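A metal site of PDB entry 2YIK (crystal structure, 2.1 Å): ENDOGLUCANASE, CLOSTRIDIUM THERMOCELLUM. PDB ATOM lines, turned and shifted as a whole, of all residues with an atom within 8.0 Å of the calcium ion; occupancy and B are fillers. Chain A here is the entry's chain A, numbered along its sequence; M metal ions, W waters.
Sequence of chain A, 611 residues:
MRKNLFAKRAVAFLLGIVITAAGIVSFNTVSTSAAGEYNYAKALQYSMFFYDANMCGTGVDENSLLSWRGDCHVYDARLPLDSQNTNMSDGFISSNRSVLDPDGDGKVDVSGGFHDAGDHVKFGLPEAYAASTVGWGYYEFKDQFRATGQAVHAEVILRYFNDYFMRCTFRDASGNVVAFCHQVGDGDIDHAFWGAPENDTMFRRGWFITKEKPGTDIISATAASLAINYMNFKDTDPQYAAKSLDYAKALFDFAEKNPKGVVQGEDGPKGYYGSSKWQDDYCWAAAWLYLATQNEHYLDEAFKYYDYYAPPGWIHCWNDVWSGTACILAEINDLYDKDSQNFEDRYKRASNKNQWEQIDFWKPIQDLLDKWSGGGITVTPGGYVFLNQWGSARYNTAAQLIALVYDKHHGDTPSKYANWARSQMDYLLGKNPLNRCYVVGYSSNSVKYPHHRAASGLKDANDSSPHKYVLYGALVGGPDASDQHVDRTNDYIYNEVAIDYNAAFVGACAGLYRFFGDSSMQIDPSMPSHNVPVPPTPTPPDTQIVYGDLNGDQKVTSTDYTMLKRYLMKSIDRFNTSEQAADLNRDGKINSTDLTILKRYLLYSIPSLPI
OD2 of Asp 337 sits close to N of Phe 343 (2.7 Å). The backbone NH (N) of Asn 342 sits close to the side-chain carboxylate (OD2) of Asp 337. OG of Ser 340 sits at hydrogen-bond distance from OD1 of Asn 342, at 3.0 Å. N of Lys 338 lies within hydrogen-bond range of O of Asn 333, at 2.9 Å.
Of the 17 residues printed, 4 come within 4 Å of the calcium ion. The nearest printed residue that does not touch the calcium ion is Gln 341 (4.3 Å).
The backbone carbonyl oxygen (O) of Asp 337 is bound to the calcium ion (2.4 Å). The calcium ion is bound by O of Ser 340 (2.5 Å). The calcium ion is bound by ND2 of Asn 333 (2.5 Å). Water W1 is bound to the calcium ion. The side-chain carboxylate (OD2) of Asp 337 binds the calcium ion (2.6 Å). OE1 of Glu 344 binds the calcium ion, 2.7 Å away. OE2 of Glu 344 binds the calcium ion, 2.7 Å away.
Water W1 bridges the backbone carbonyl oxygen of Lys 338 (2.8 Å) and the side-chain amide oxygen of Asn 333 (3.1 Å).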
ATOM      1  N   ALA A 330      33.351  12.819 -19.822  1.00  0.00           N
ATOM      2  CA  ALA A 330      32.248  12.430 -18.945  1.00  0.00           C
ATOM      3  C   ALA A 330      32.696  12.472 -17.486  1.00  0.00           C
ATOM      4  O   ALA A 330      31.940  12.899 -16.611  1.00  0.00           O
ATOM      5  CB  ALA A 330      31.742  11.045 -19.317  1.00  0.00           C
ATOM      6  N   ILE A 332      35.004  14.353 -16.347  1.00  0.00           N
ATOM      7  CA  ILE A 332      35.194  15.767 -16.056  1.00  0.00           C
ATOM      8  C   ILE A 332      33.840  16.366 -15.670  1.00  0.00           C
ATOM      9  O   ILE A 332      33.730  17.144 -14.727  1.00  0.00           O
ATOM     10  CB  ILE A 332      35.763  16.492 -17.300  1.00  0.00           C
ATOM     11  CG1 ILE A 332      37.270  16.222 -17.392  1.00  0.00           C
ATOM     12  CG2 ILE A 332      35.453  17.989 -17.244  1.00  0.00           C
ATOM     13  CD1 ILE A 332      37.884  16.645 -18.703  1.00  0.00           C
ATOM     14  N   ASN A 333      32.807  15.977 -16.413  1.00  0.00           N
ATOM     15  CA  ASN A 333      31.470  16.463 -16.135  1.00  0.00           C
ATOM     16  C   ASN A 333      30.974  15.993 -14.775  1.00  0.00           C
ATOM     17  O   ASN A 333      30.353  16.758 -14.042  1.00  0.00           O
ATOM     18  CB  ASN A 333      30.484  16.005 -17.201  1.00  0.00           C
ATOM     19  CG  ASN A 333      29.075  16.455 -16.893  1.00  0.00           C
ATOM     20  OD1 ASN A 333      28.200  15.658 -16.548  1.00  0.00           O
ATOM     21  ND2 ASN A 333      28.864  17.755 -16.996  1.00  0.00           N
ATOM     22  N   ASP A 334      31.243  14.736 -14.439  1.00  0.00           N
ATOM     23  CA  ASP A 334      30.822  14.169 -13.163  1.00  0.00           C
ATOM     24  C   ASP A 334      31.512  14.871 -12.000  1.00  0.00           C
ATOM     25  O   ASP A 334      30.889  15.153 -10.981  1.00  0.00           O
ATOM     26  CB  ASP A 334      31.135  12.671 -13.087  1.00  0.00           C
ATOM     27  CG  ASP A 334      30.210  11.826 -13.939  1.00  0.00           C
ATOM     28  OD1 ASP A 334      29.138  12.317 -14.368  1.00  0.00           O
ATOM     29  OD2 ASP A 334      30.537  10.631 -14.169  1.00  0.00           O
ATOM     30  N   TYR A 336      33.098  18.026 -11.967  1.00  0.00           N
ATOM     31  CA  TYR A 336      32.876  19.454 -11.857  1.00  0.00           C
ATOM     32  C   TYR A 336      31.543  20.063 -12.279  1.00  0.00           C
ATOM     33  O   TYR A 336      31.315  21.235 -12.029  1.00  0.00           O
ATOM     34  CB  TYR A 336      33.994  20.152 -12.642  1.00  0.00           C
ATOM     35  CG  TYR A 336      35.364  19.729 -12.177  1.00  0.00           C
ATOM     36  CD1 TYR A 336      35.841  20.088 -10.919  1.00  0.00           C
ATOM     37  CD2 TYR A 336      36.189  18.939 -12.986  1.00  0.00           C
ATOM     38  CE1 TYR A 336      37.092  19.686 -10.467  1.00  0.00           C
ATOM     39  CE2 TYR A 336      37.450  18.528 -12.545  1.00  0.00           C
ATOM     40  CZ  TYR A 336      37.897  18.907 -11.284  1.00  0.00           C
ATOM     41  OH  TYR A 336      39.147  18.534 -10.827  1.00  0.00           O
ATOM     42  N   ASP A 337      30.667  19.294 -12.914  1.00  0.00           N
ATOM     43  CA  ASP A 337      29.405  19.857 -13.361  1.00  0.00           C
ATOM     44  C   ASP A 337      28.264  18.829 -13.290  1.00  0.00           C
ATOM     45  O   ASP A 337      27.311  18.889 -14.047  1.00  0.00           O
ATOM     46  CB  ASP A 337      29.584  20.367 -14.801  1.00  0.00           C
ATOM     47  CG  ASP A 337      28.471  21.277 -15.255  1.00  0.00           C
ATOM     48  OD1 ASP A 337      28.120  22.228 -14.519  1.00  0.00           O
ATOM     49  OD2 ASP A 337      27.957  21.067 -16.369  1.00  0.00           O
ATOM     50  N   LYS A 338      28.352  17.906 -12.340  1.00  0.00           N
ATOM     51  CA  LYS A 338      27.366  16.842 -12.166  1.00  0.00           C
ATOM     52  C   LYS A 338      25.899  17.278 -12.096  1.00  0.00           C
ATOM     53  O   LYS A 338      25.046  16.736 -12.814  1.00  0.00           O
ATOM     54  CB  LYS A 338      27.718  16.045 -10.909  1.00  0.00           C
ATOM     55  CG  LYS A 338      26.754  14.919 -10.541  1.00  0.00           C
ATOM     56  CD  LYS A 338      27.009  13.654 -11.343  1.00  0.00           C
ATOM     57  CE  LYS A 338      26.732  12.417 -10.483  1.00  0.00           C
ATOM     58  NZ  LYS A 338      27.073  11.150 -11.200  1.00  0.00           N
ATOM     59  N   ASP A 339      25.592  18.260 -11.241  1.00  0.00           N
ATOM     60  CA  ASP A 339      24.210  18.701 -11.064  1.00  0.00           C
ATOM     61  C   ASP A 339      23.703  19.917 -11.855  1.00  0.00           C
ATOM     62  O   ASP A 339      22.758  20.576 -11.429  1.00  0.00           O
ATOM     63  CB  ASP A 339      23.954  18.941  -9.567  1.00  0.00           C
ATOM     64  CG  ASP A 339      24.317  17.733  -8.711  1.00  0.00           C
ATOM     65  OD1 ASP A 339      23.910  16.600  -9.068  1.00  0.00           O
ATOM     66  OD2 ASP A 339      24.997  17.919  -7.684  1.00  0.00           O
ATOM     67  N   SER A 340      24.309  20.220 -12.993  1.00  0.00           N
ATOM     68  CA  SER A 340      23.833  21.346 -13.786  1.00  0.00           C
ATOM     69  C   SER A 340      24.077  21.072 -15.260  1.00  0.00           C
ATOM     70  O   SER A 340      24.709  20.090 -15.591  1.00  0.00           O
ATOM     71  CB  SER A 340      24.516  22.640 -13.340  1.00  0.00           C
ATOM     72  OG  SER A 340      25.626  22.970 -14.165  1.00  0.00           O
ATOM     73  N   GLN A 341      23.567  21.919 -16.151  1.00  0.00           N
ATOM     74  CA  GLN A 341      23.750  21.720 -17.594  1.00  0.00           C
ATOM     75  C   GLN A 341      24.789  22.637 -18.236  1.00  0.00           C
ATOM     76  O   GLN A 341      24.869  22.726 -19.465  1.00  0.00           O
ATOM     77  CB  GLN A 341      22.413  21.912 -18.318  1.00  0.00           C
ATOM     78  CG  GLN A 341      21.419  20.769 -18.157  1.00  0.00           C
ATOM     79  CD  GLN A 341      21.926  19.468 -18.781  1.00  0.00           C
ATOM     80  OE1 GLN A 341      22.326  18.549 -18.079  1.00  0.00           O
ATOM     81  NE2 GLN A 341      21.922  19.400 -20.110  1.00  0.00           N
ATOM     82  N   ASN A 342      25.596  23.315 -17.417  1.00  0.00           N
ATOM     83  CA  ASN A 342      26.599  24.233 -17.939  1.00  0.00           C
ATOM     84  C   ASN A 342      27.544  23.663 -18.979  1.00  0.00           C
ATOM     85  O   ASN A 342      27.685  24.235 -20.056  1.00  0.00           O
ATOM     86  CB  ASN A 342      27.420  24.836 -16.786  1.00  0.00           C
ATOM     87  CG  ASN A 342      26.669  25.936 -16.065  1.00  0.00           C
ATOM     88  OD1 ASN A 342      26.291  25.783 -14.902  1.00  0.00           O
ATOM     89  ND2 ASN A 342      26.448  27.048 -16.757  1.00  0.00           N
ATOM     90  N   PHE A 343      28.205  22.538 -18.673  1.00  0.00           N
ATOM     91  CA  PHE A 343      29.136  21.935 -19.629  1.00  0.00           C
ATOM     92  C   PHE A 343      28.400  21.471 -20.887  1.00  0.00           C
ATOM     93  O   PHE A 343      28.884  21.667 -21.998  1.00  0.00           O
ATOM     94  CB  PHE A 343      29.870  20.745 -18.985  1.00  0.00           C
ATOM     95  CG  PHE A 343      30.951  21.145 -17.995  1.00  0.00           C
ATOM     96  CD1 PHE A 343      31.030  22.443 -17.496  1.00  0.00           C
ATOM     97  CD2 PHE A 343      31.864  20.191 -17.538  1.00  0.00           C
ATOM     98  CE1 PHE A 343      32.013  22.788 -16.550  1.00  0.00           C
ATOM     99  CE2 PHE A 343      32.837  20.516 -16.595  1.00  0.00           C
ATOM    100  CZ  PHE A 343      32.916  21.824 -16.094  1.00  0.00           C
ATOM    101  N   GLU A 344      27.232  20.860 -20.709  1.00  0.00           N
ATOM    102  CA  GLU A 344      26.460  20.388 -21.858  1.00  0.00           C
ATOM    103  C   GLU A 344      26.070  21.545 -22.774  1.00  0.00           C
ATOM    104  O   GLU A 344      26.201  21.462 -23.998  1.00  0.00           O
ATOM    105  CB  GLU A 344      25.189  19.660 -21.399  1.00  0.00           C
ATOM    106  CG  GLU A 344      25.432  18.319 -20.734  1.00  0.00           C
ATOM    107  CD  GLU A 344      25.821  18.465 -19.291  1.00  0.00           C
ATOM    108  OE1 GLU A 344      26.034  19.621 -18.849  1.00  0.00           O
ATOM    109  OE2 GLU A 344      25.911  17.431 -18.593  1.00  0.00           O
ATOM    110  N   ASP A 345      25.565  22.629 -22.186  1.00  0.00           N
ATOM    111  CA  ASP A 345      25.159  23.775 -22.973  1.00  0.00           C
ATOM    112  C   ASP A 345      26.339  24.491 -23.610  1.00  0.00           C
ATOM    113  O   ASP A 345      26.210  25.041 -24.703  1.00  0.00           O
ATOM    114  CB  ASP A 345      24.322  24.732 -22.127  1.00  0.00           C
ATOM    115  CG  ASP A 345      22.983  24.134 -21.732  1.00  0.00           C
ATOM    116  OD1 ASP A 345      22.569  23.152 -22.389  1.00  0.00           O
ATOM    117  OD2 ASP A 345      22.353  24.652 -20.786  1.00  0.00           O
ATOM    118  N   ILE A 359      22.232  16.129 -24.655  1.00  0.00           N
ATOM    119  CA  ILE A 359      23.637  15.817 -24.495  1.00  0.00           C
ATOM    120  C   ILE A 359      23.861  15.259 -23.104  1.00  0.00           C
ATOM    121  O   ILE A 359      23.538  15.903 -22.102  1.00  0.00           O
ATOM    122  CB  ILE A 359      24.551  17.069 -24.652  1.00  0.00           C
ATOM    123  CG1 ILE A 359      24.601  17.529 -26.106  1.00  0.00           C
ATOM    124  CG2 ILE A 359      25.960  16.757 -24.178  1.00  0.00           C
ATOM    125  CD1 ILE A 359      23.290  18.065 -26.580  1.00  0.00           C
ATOM    126  N   ASP A 360      24.395  14.042 -23.053  1.00  0.00           N
ATOM    127  CA  ASP A 360      24.726  13.366 -21.798  1.00  0.00           C
ATOM    128  C   ASP A 360      26.096  12.797 -22.117  1.00  0.00           C
ATOM    129  O   ASP A 360      26.230  11.877 -22.930  1.00  0.00           O
ATOM    130  CB  ASP A 360      23.713  12.267 -21.468  1.00  0.00           C
ATOM    131  CG  ASP A 360      24.095  11.462 -20.222  1.00  0.00           C
ATOM    132  OD1 ASP A 360      25.301  11.363 -19.895  1.00  0.00           O
ATOM    133  OD2 ASP A 360      23.185  10.910 -19.575  1.00  0.00           O
ATOM    134  N   PHE A 361      27.113  13.343 -21.472  1.00  0.00           N
ATOM    135  CA  PHE A 361      28.479  12.915 -21.728  1.00  0.00           C
ATOM    136  C   PHE A 361      28.763  11.409 -21.665  1.00  0.00           C
ATOM    137  O   PHE A 361      29.622  10.932 -22.401  1.00  0.00           O
ATOM    138  CB  PHE A 361      29.444  13.729 -20.859  1.00  0.00           C
ATOM    139  CG  PHE A 361      29.580  15.171 -21.307  1.00  0.00           C
ATOM    140  CD1 PHE A 361      30.179  15.477 -22.526  1.00  0.00           C
ATOM    141  CD2 PHE A 361      29.056  16.216 -20.544  1.00  0.00           C
ATOM    142  CE1 PHE A 361      30.247  16.799 -22.987  1.00  0.00           C
ATOM    143  CE2 PHE A 361      29.113  17.546 -20.994  1.00  0.00           C
ATOM    144  CZ  PHE A 361      29.713  17.833 -22.216  1.00  0.00           C
HETATM  145 CA    CA M   1      26.626  18.784 -16.390  1.00  0.00          CA
HETATM  146  O   HOH W   1      25.442  16.595 -15.536  1.00  0.00           O
